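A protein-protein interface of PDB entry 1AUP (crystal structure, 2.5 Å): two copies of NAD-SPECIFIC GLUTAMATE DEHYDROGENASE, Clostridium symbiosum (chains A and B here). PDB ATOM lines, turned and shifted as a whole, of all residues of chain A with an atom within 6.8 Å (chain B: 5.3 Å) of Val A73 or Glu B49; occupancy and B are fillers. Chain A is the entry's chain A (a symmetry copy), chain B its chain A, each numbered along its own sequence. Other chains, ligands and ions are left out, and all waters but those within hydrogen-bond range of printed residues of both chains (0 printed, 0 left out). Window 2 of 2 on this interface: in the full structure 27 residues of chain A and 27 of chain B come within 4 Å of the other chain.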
ATOM      1  N   ARG A  61       7.635 -28.811   0.428  1.00  0.00           N
ATOM      2  CA  ARG A  61       7.505 -29.150  -0.975  1.00  0.00           C
ATOM      3  C   ARG A  61       7.783 -30.639  -1.163  1.00  0.00           C
ATOM      4  O   ARG A  61       8.764 -31.156  -0.660  1.00  0.00           O
ATOM      5  CB  ARG A  61       8.500 -28.322  -1.803  1.00  0.00           C
ATOM      6  CG  ARG A  61       8.437 -28.584  -3.324  1.00  0.00           C
ATOM      7  CD  ARG A  61       9.675 -28.066  -4.068  1.00  0.00           C
ATOM      8  NE  ARG A  61       9.937 -26.644  -3.853  1.00  0.00           N
ATOM      9  CZ  ARG A  61      11.103 -26.054  -4.101  1.00  0.00           C
ATOM     10  NH1 ARG A  61      12.128 -26.758  -4.559  1.00  0.00           N
ATOM     11  NH2 ARG A  61      11.246 -24.766  -3.888  1.00  0.00           N
ATOM     12  N   VAL A  62       6.920 -31.325  -1.891  1.00  0.00           N
ATOM     13  CA  VAL A  62       7.130 -32.741  -2.140  1.00  0.00           C
ATOM     14  C   VAL A  62       7.090 -33.031  -3.615  1.00  0.00           C
ATOM     15  O   VAL A  62       6.047 -33.302  -4.183  1.00  0.00           O
ATOM     16  CB  VAL A  62       6.100 -33.633  -1.422  1.00  0.00           C
ATOM     17  CG1 VAL A  62       6.649 -35.064  -1.307  1.00  0.00           C
ATOM     18  CG2 VAL A  62       5.750 -33.058  -0.024  1.00  0.00           C
ATOM     19  N   PRO A  63       8.239 -32.944  -4.237  1.00  0.00           N
ATOM     20  CA  PRO A  63       8.337 -33.206  -5.656  1.00  0.00           C
ATOM     21  C   PRO A  63       8.512 -34.694  -5.854  1.00  0.00           C
ATOM     22  O   PRO A  63       9.255 -35.349  -5.102  1.00  0.00           O
ATOM     23  CB  PRO A  63       9.605 -32.430  -6.090  1.00  0.00           C
ATOM     24  CG  PRO A  63      10.289 -31.983  -4.834  1.00  0.00           C
ATOM     25  CD  PRO A  63       9.477 -32.404  -3.651  1.00  0.00           C
ATOM     26  N   TRP A  64       7.812 -35.237  -6.851  1.00  0.00           N
ATOM     27  CA  TRP A  64       7.887 -36.661  -7.162  1.00  0.00           C
ATOM     28  C   TRP A  64       7.671 -36.972  -8.649  1.00  0.00           C
ATOM     29  O   TRP A  64       7.106 -36.172  -9.394  1.00  0.00           O
ATOM     30  CB  TRP A  64       6.920 -37.464  -6.282  1.00  0.00           C
ATOM     31  CG  TRP A  64       5.513 -37.105  -6.485  1.00  0.00           C
ATOM     32  CD1 TRP A  64       4.852 -36.029  -5.964  1.00  0.00           C
ATOM     33  CD2 TRP A  64       4.579 -37.786  -7.320  1.00  0.00           C
ATOM     34  NE1 TRP A  64       3.555 -36.002  -6.425  1.00  0.00           N
ATOM     35  CE2 TRP A  64       3.362 -37.079  -7.252  1.00  0.00           C
ATOM     36  CE3 TRP A  64       4.659 -38.914  -8.134  1.00  0.00           C
ATOM     37  CZ2 TRP A  64       2.227 -37.481  -7.955  1.00  0.00           C
ATOM     38  CZ3 TRP A  64       3.519 -39.325  -8.811  1.00  0.00           C
ATOM     39  CH2 TRP A  64       2.328 -38.609  -8.723  1.00  0.00           C
ATOM     40  N   VAL A  71       7.154 -35.295 -13.651  1.00  0.00           N
ATOM     41  CA  VAL A  71       7.340 -34.818 -12.278  1.00  0.00           C
ATOM     42  C   VAL A  71       6.112 -34.054 -11.755  1.00  0.00           C
ATOM     43  O   VAL A  71       5.499 -33.268 -12.484  1.00  0.00           O
ATOM     44  CB  VAL A  71       8.593 -33.932 -12.166  1.00  0.00           C
ATOM     45  CG1 VAL A  71       8.813 -33.511 -10.740  1.00  0.00           C
ATOM     46  CG2 VAL A  71       9.809 -34.679 -12.674  1.00  0.00           C
ATOM     47  N   HIS A  72       5.743 -34.313 -10.498  1.00  0.00           N
ATOM     48  CA  HIS A  72       4.602 -33.644  -9.853  1.00  0.00           C
ATOM     49  C   HIS A  72       5.106 -33.137  -8.548  1.00  0.00           C
ATOM     50  O   HIS A  72       6.063 -33.668  -7.990  1.00  0.00           O
ATOM     51  CB  HIS A  72       3.459 -34.633  -9.578  1.00  0.00           C
ATOM     52  CG  HIS A  72       3.052 -35.409 -10.775  1.00  0.00           C
ATOM     53  ND1 HIS A  72       1.884 -35.162 -11.462  1.00  0.00           N
ATOM     54  CD2 HIS A  72       3.699 -36.382 -11.469  1.00  0.00           C
ATOM     55  CE1 HIS A  72       1.820 -35.963 -12.514  1.00  0.00           C
ATOM     56  NE2 HIS A  72       2.907 -36.715 -12.539  1.00  0.00           N
ATOM     57  N   VAL A  73       4.491 -32.092  -8.060  1.00  0.00           N
ATOM     58  CA  VAL A  73       4.925 -31.525  -6.837  1.00  0.00           C
ATOM     59  C   VAL A  73       3.698 -31.203  -6.012  1.00  0.00           C
ATOM     60  O   VAL A  73       2.709 -30.700  -6.526  1.00  0.00           O
ATOM     61  CB  VAL A  73       5.871 -30.322  -7.078  1.00  0.00           C
ATOM     62  CG1 VAL A  73       5.296 -29.379  -8.081  1.00  0.00           C
ATOM     63  CG2 VAL A  73       6.172 -29.626  -5.804  1.00  0.00           C
ATOM     64  N   ASN A  74       3.714 -31.666  -4.770  1.00  0.00           N
ATOM     65  CA  ASN A  74       2.601 -31.491  -3.862  1.00  0.00           C
ATOM     66  C   ASN A  74       3.118 -30.818  -2.618  1.00  0.00           C
ATOM     67  O   ASN A  74       4.312 -30.554  -2.510  1.00  0.00           O
ATOM     68  CB  ASN A  74       2.007 -32.858  -3.508  1.00  0.00           C
ATOM     69  CG  ASN A  74       1.287 -33.475  -4.663  1.00  0.00           C
ATOM     70  OD1 ASN A  74       1.870 -34.218  -5.446  1.00  0.00           O
ATOM     71  ND2 ASN A  74       0.040 -33.102  -4.833  1.00  0.00           N
ATOM     72  N   THR A  75       2.231 -30.565  -1.662  1.00  0.00           N
ATOM     73  CA  THR A  75       2.633 -29.954  -0.417  1.00  0.00           C
ATOM     74  C   THR A  75       2.415 -30.911   0.760  1.00  0.00           C
ATOM     75  O   THR A  75       1.357 -31.521   0.890  1.00  0.00           O
ATOM     76  CB  THR A  75       1.900 -28.625  -0.185  1.00  0.00           C
ATOM     77  OG1 THR A  75       2.156 -27.758  -1.289  1.00  0.00           O
ATOM     78  CG2 THR A  75       2.380 -27.937   1.123  1.00  0.00           C
ATOM     79  N   ASP A 129      -1.775 -32.720  -0.128  1.00  0.00           N
ATOM     80  CA  ASP A 129      -2.862 -32.532  -1.076  1.00  0.00           C
ATOM     81  C   ASP A 129      -2.685 -33.538  -2.213  1.00  0.00           C
ATOM     82  O   ASP A 129      -3.292 -33.431  -3.293  1.00  0.00           O
ATOM     83  CB  ASP A 129      -2.826 -31.120  -1.616  1.00  0.00           C
ATOM     84  CG  ASP A 129      -1.474 -30.761  -2.197  1.00  0.00           C
ATOM     85  OD1 ASP A 129      -0.610 -31.662  -2.294  1.00  0.00           O
ATOM     86  OD2 ASP A 129      -1.305 -29.599  -2.634  1.00  0.00           O
ATOM     87  N   PHE A 143       6.115 -41.297  -3.977  1.00  0.00           N
ATOM     88  CA  PHE A 143       5.642 -40.122  -3.299  1.00  0.00           C
ATOM     89  C   PHE A 143       5.919 -40.215  -1.826  1.00  0.00           C
ATOM     90  O   PHE A 143       6.444 -39.287  -1.237  1.00  0.00           O
ATOM     91  CB  PHE A 143       4.182 -39.905  -3.514  1.00  0.00           C
ATOM     92  CG  PHE A 143       3.617 -38.904  -2.601  1.00  0.00           C
ATOM     93  CD1 PHE A 143       3.750 -37.552  -2.878  1.00  0.00           C
ATOM     94  CD2 PHE A 143       3.075 -39.288  -1.403  1.00  0.00           C
ATOM     95  CE1 PHE A 143       3.288 -36.605  -2.004  1.00  0.00           C
ATOM     96  CE2 PHE A 143       2.622 -38.353  -0.512  1.00  0.00           C
ATOM     97  CZ  PHE A 143       2.717 -36.999  -0.816  1.00  0.00           C
ATOM     98  N   TYR B   3       3.267 -22.323 -20.623  1.00  0.00           N
ATOM     99  CA  TYR B   3       3.705 -22.954 -19.339  1.00  0.00           C
ATOM    100  C   TYR B   3       3.674 -21.845 -18.280  1.00  0.00           C
ATOM    101  O   TYR B   3       2.954 -21.925 -17.276  1.00  0.00           O
ATOM    102  CB  TYR B   3       5.153 -23.514 -19.507  1.00  0.00           C
ATOM    103  CG  TYR B   3       5.879 -24.102 -18.252  1.00  0.00           C
ATOM    104  CD1 TYR B   3       5.180 -24.642 -17.177  1.00  0.00           C
ATOM    105  CD2 TYR B   3       7.278 -24.190 -18.220  1.00  0.00           C
ATOM    106  CE1 TYR B   3       5.873 -25.203 -16.067  1.00  0.00           C
ATOM    107  CE2 TYR B   3       7.964 -24.746 -17.134  1.00  0.00           C
ATOM    108  CZ  TYR B   3       7.266 -25.260 -16.074  1.00  0.00           C
ATOM    109  OH  TYR B   3       7.983 -25.777 -15.004  1.00  0.00           O
ATOM    110  N   ARG B   6       0.183 -20.560 -17.408  1.00  0.00           N
ATOM    111  CA  ARG B   6      -0.585 -21.562 -16.691  1.00  0.00           C
ATOM    112  C   ARG B   6      -0.253 -21.498 -15.202  1.00  0.00           C
ATOM    113  O   ARG B   6      -1.104 -21.178 -14.361  1.00  0.00           O
ATOM    114  CB  ARG B   6      -0.242 -22.938 -17.251  1.00  0.00           C
ATOM    115  CG  ARG B   6      -0.565 -24.081 -16.366  1.00  0.00           C
ATOM    116  CD  ARG B   6      -0.460 -25.391 -17.139  1.00  0.00           C
ATOM    117  NE  ARG B   6       0.921 -25.788 -17.389  1.00  0.00           N
ATOM    118  CZ  ARG B   6       1.716 -26.362 -16.489  1.00  0.00           C
ATOM    119  NH1 ARG B   6       1.287 -26.595 -15.245  1.00  0.00           N
ATOM    120  NH2 ARG B   6       2.953 -26.691 -16.826  1.00  0.00           N
ATOM    121  N   VAL B   7       0.996 -21.801 -14.889  1.00  0.00           N
ATOM    122  CA  VAL B   7       1.480 -21.777 -13.527  1.00  0.00           C
ATOM    123  C   VAL B   7       0.985 -20.543 -12.790  1.00  0.00           C
ATOM    124  O   VAL B   7       0.502 -20.640 -11.666  1.00  0.00           O
ATOM    125  CB  VAL B   7       3.019 -21.817 -13.506  1.00  0.00           C
ATOM    126  CG1 VAL B   7       3.544 -21.624 -12.103  1.00  0.00           C
ATOM    127  CG2 VAL B   7       3.539 -23.101 -14.140  1.00  0.00           C
ATOM    128  N   GLU B  10      -2.470 -20.967 -11.988  1.00  0.00           N
ATOM    129  CA  GLU B  10      -2.608 -21.968 -10.939  1.00  0.00           C
ATOM    130  C   GLU B  10      -2.333 -21.341  -9.572  1.00  0.00           C
ATOM    131  O   GLU B  10      -3.119 -21.495  -8.645  1.00  0.00           O
ATOM    132  CB  GLU B  10      -1.665 -23.146 -11.214  1.00  0.00           C
ATOM    133  CG  GLU B  10      -2.119 -24.030 -12.403  1.00  0.00           C
ATOM    134  CD  GLU B  10      -1.133 -25.135 -12.729  1.00  0.00           C
ATOM    135  OE1 GLU B  10      -0.082 -25.217 -12.057  1.00  0.00           O
ATOM    136  OE2 GLU B  10      -1.417 -25.928 -13.648  1.00  0.00           O
ATOM    137  N   GLU B  43       9.971 -27.501 -18.218  1.00  0.00           N
ATOM    138  CA  GLU B  43       8.641 -28.024 -17.995  1.00  0.00           C
ATOM    139  C   GLU B  43       8.676 -29.510 -17.693  1.00  0.00           C
ATOM    140  O   GLU B  43       7.915 -30.003 -16.862  1.00  0.00           O
ATOM    141  CB  GLU B  43       7.735 -27.744 -19.185  1.00  0.00           C
ATOM    142  CG  GLU B  43       6.273 -27.517 -18.807  1.00  0.00           C
ATOM    143  CD  GLU B  43       5.355 -27.489 -20.018  1.00  0.00           C
ATOM    144  OE1 GLU B  43       5.869 -27.516 -21.157  1.00  0.00           O
ATOM    145  OE2 GLU B  43       4.114 -27.448 -19.828  1.00  0.00           O
ATOM    146  N   ALA B  46       8.962 -29.941 -14.204  1.00  0.00           N
ATOM    147  CA  ALA B  46       8.065 -29.070 -13.428  1.00  0.00           C
ATOM    148  C   ALA B  46       8.846 -28.063 -12.627  1.00  0.00           C
ATOM    149  O   ALA B  46       8.658 -27.930 -11.413  1.00  0.00           O
ATOM    150  CB  ALA B  46       7.202 -29.925 -12.483  1.00  0.00           C
ATOM    151  N   LEU B  47       9.726 -27.350 -13.294  1.00  0.00           N
ATOM    152  CA  LEU B  47      10.573 -26.422 -12.603  1.00  0.00           C
ATOM    153  C   LEU B  47       9.823 -25.262 -11.985  1.00  0.00           C
ATOM    154  O   LEU B  47      10.006 -24.935 -10.837  1.00  0.00           O
ATOM    155  CB  LEU B  47      11.639 -25.904 -13.515  1.00  0.00           C
ATOM    156  CG  LEU B  47      12.497 -24.928 -12.755  1.00  0.00           C
ATOM    157  CD1 LEU B  47      12.601 -25.384 -11.318  1.00  0.00           C
ATOM    158  CD2 LEU B  47      13.815 -24.883 -13.359  1.00  0.00           C
ATOM    159  N   LEU B  48       8.994 -24.615 -12.764  1.00  0.00           N
ATOM    160  CA  LEU B  48       8.270 -23.493 -12.246  1.00  0.00           C
ATOM    161  C   LEU B  48       7.404 -23.925 -11.076  1.00  0.00           C
ATOM    162  O   LEU B  48       7.371 -23.282 -10.013  1.00  0.00           O
ATOM    163  CB  LEU B  48       7.454 -22.876 -13.352  1.00  0.00           C
ATOM    164  CG  LEU B  48       8.331 -22.299 -14.469  1.00  0.00           C
ATOM    165  CD1 LEU B  48       7.464 -21.707 -15.569  1.00  0.00           C
ATOM    166  CD2 LEU B  48       9.235 -21.233 -13.882  1.00  0.00           C
ATOM    167  N   GLU B  49       6.723 -25.041 -11.264  1.00  0.00           N
ATOM    168  CA  GLU B  49       5.852 -25.594 -10.243  1.00  0.00           C
ATOM    169  C   GLU B  49       6.572 -25.881  -8.888  1.00  0.00           C
ATOM    170  O   GLU B  49       5.990 -25.729  -7.844  1.00  0.00           O
ATOM    171  CB  GLU B  49       5.159 -26.840 -10.774  1.00  0.00           C
ATOM    172  CG  GLU B  49       4.311 -26.613 -12.036  1.00  0.00           C
ATOM    173  CD  GLU B  49       5.020 -27.066 -13.277  1.00  0.00           C
ATOM    174  OE1 GLU B  49       6.235 -26.792 -13.363  1.00  0.00           O
ATOM    175  OE2 GLU B  49       4.377 -27.726 -14.144  1.00  0.00           O
ATOM    176  N   ARG B  50       7.836 -26.268  -8.931  1.00  0.00           N
ATOM    177  CA  ARG B  50       8.597 -26.500  -7.704  1.00  0.00           C
ATOM    178  C   ARG B  50       9.022 -25.154  -7.118  1.00  0.00           C
ATOM    179  O   ARG B  50       9.073 -24.966  -5.906  1.00  0.00           O
ATOM    180  CB  ARG B  50       9.882 -27.284  -8.014  1.00  0.00           C
ATOM    181  CG  ARG B  50       9.689 -28.682  -8.589  1.00  0.00           C
ATOM    182  CD  ARG B  50      11.021 -29.485  -8.482  1.00  0.00           C
ATOM    183  NE  ARG B  50      11.613 -29.806  -9.785  1.00  0.00           N
ATOM    184  CZ  ARG B  50      12.925 -29.915 -10.011  1.00  0.00           C
ATOM    185  NH1 ARG B  50      13.794 -29.745  -9.016  1.00  0.00           N
ATOM    186  NH2 ARG B  50      13.374 -30.234 -11.226  1.00  0.00           N
ATOM    187  N   MET B  51       9.400 -24.240  -7.993  1.00  0.00           N
ATOM    188  CA  MET B  51       9.935 -22.971  -7.559  1.00  0.00           C
ATOM    189  C   MET B  51       9.008 -22.157  -6.747  1.00  0.00           C
ATOM    190  O   MET B  51       9.437 -21.439  -5.849  1.00  0.00           O
ATOM    191  CB  MET B  51      10.457 -22.165  -8.730  1.00  0.00           C
ATOM    192  CG  MET B  51      11.937 -22.361  -8.992  1.00  0.00           C
ATOM    193  SD  MET B  51      12.567 -21.195 -10.201  1.00  0.00           S
ATOM    194  CE  MET B  51      11.105 -20.041 -10.366  1.00  0.00           C
ATOM    195  N   VAL B  52       7.733 -22.215  -7.079  1.00  0.00           N
ATOM    196  CA  VAL B  52       6.774 -21.404  -6.375  1.00  0.00           C
ATOM    197  C   VAL B  52       6.380 -21.924  -4.999  1.00  0.00           C
ATOM    198  O   VAL B  52       5.733 -21.228  -4.228  1.00  0.00           O
ATOM    199  CB  VAL B  52       5.617 -21.085  -7.233  1.00  0.00           C
ATOM    200  CG1 VAL B  52       6.126 -20.530  -8.546  1.00  0.00           C
ATOM    201  CG2 VAL B  52       4.768 -22.324  -7.471  1.00  0.00           C
ATOM    202  N   ILE B  53       6.828 -23.130  -4.671  1.00  0.00           N
ATOM    203  CA  ILE B  53       6.574 -23.699  -3.352  1.00  0.00           C
ATOM    204  C   ILE B  53       7.858 -23.692  -2.553  1.00  0.00           C
ATOM    205  O   ILE B  53       8.870 -24.261  -2.963  1.00  0.00           O
ATOM    206  CB  ILE B  53       6.033 -25.146  -3.422  1.00  0.00           C
ATOM    207  CG1 ILE B  53       4.737 -25.196  -4.226  1.00  0.00           C
ATOM    208  CG2 ILE B  53       5.768 -25.685  -2.007  1.00  0.00           C
ATOM    209  CD1 ILE B  53       4.224 -26.590  -4.419  1.00  0.00           C
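The backbone carbonyl oxygen (O) of Arg B50 sits at hydrogen-bond distance from the guanidinium group (NE) of Arg A61, 2.8 Å away.
The backbone carbonyl oxygen of Ile B53 is in hydrogen-bond range of the guanidinium group of Arg A61 (2.6 Å).
The side-chain hydroxyl (OH) of Tyr B3 sits at hydrogen-bond distance from the side-chain carboxylate (OE1) of Glu B49, 2.6 Å away.
The side-chain carboxylate (OE2) of Glu B49 is in salt-bridge range of the guanidinium group (NH2) of Arg B6 (3.2 Å).
The side-chain carboxylate (OD1) of Asp A129 lies within hydrogen-bond range of the backbone NH (N) of Thr A75 (3.1 Å).
Among the printed residues, pairs that only touch across the chains: Val A71 with Ala B46 (3.8 Å), Val A73 with Glu B49 (3.7 Å), Val A73 with Ile B53 (3.9 Å) and Thr A75 with Ile B53 (3.9 Å).
Printed residues of chain B within 4 Å of Arg A61: Arg B50 (2.8 Å) and Ile B53 (2.6 Å).
Printed residues of chain B within 4 Å of Val A73: Glu B49 (3.7 Å) and Ile B53 (3.9 Å).
Of the printed residues of chain B, Thr A75 touches Ile B53 (3.9 Å).
Arg B6 touches none of the printed residues of chain A.
Of the printed residues of chain A, Ala B46 touches Val A71 (3.8 Å).
Of the printed residues of chain A, Glu B49 touches Val A73.
Of the printed residues of chain A, Ile B53 touches Arg A61, Val A73 and Thr A75.
Hydrophobic or aromatic side chains of chain A within 4 Å of the printed part of chain B: Val A73.
Printed residues of chain B that touch a printed residue of chain A: Ala B46, Glu B49, Arg B50 and Ile B53.
Among the printed residues, 6 pairs touch across the chains.
Among the printed residues, no Asp or Glu carboxylate lies within 4 Å of a Lys or Arg side-chain nitrogen of the other chain.
No position is printed for both chains.
Of the 6 pairs that touch across the chains among the printed residues, none has its exchanged pair printed and touching as well.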
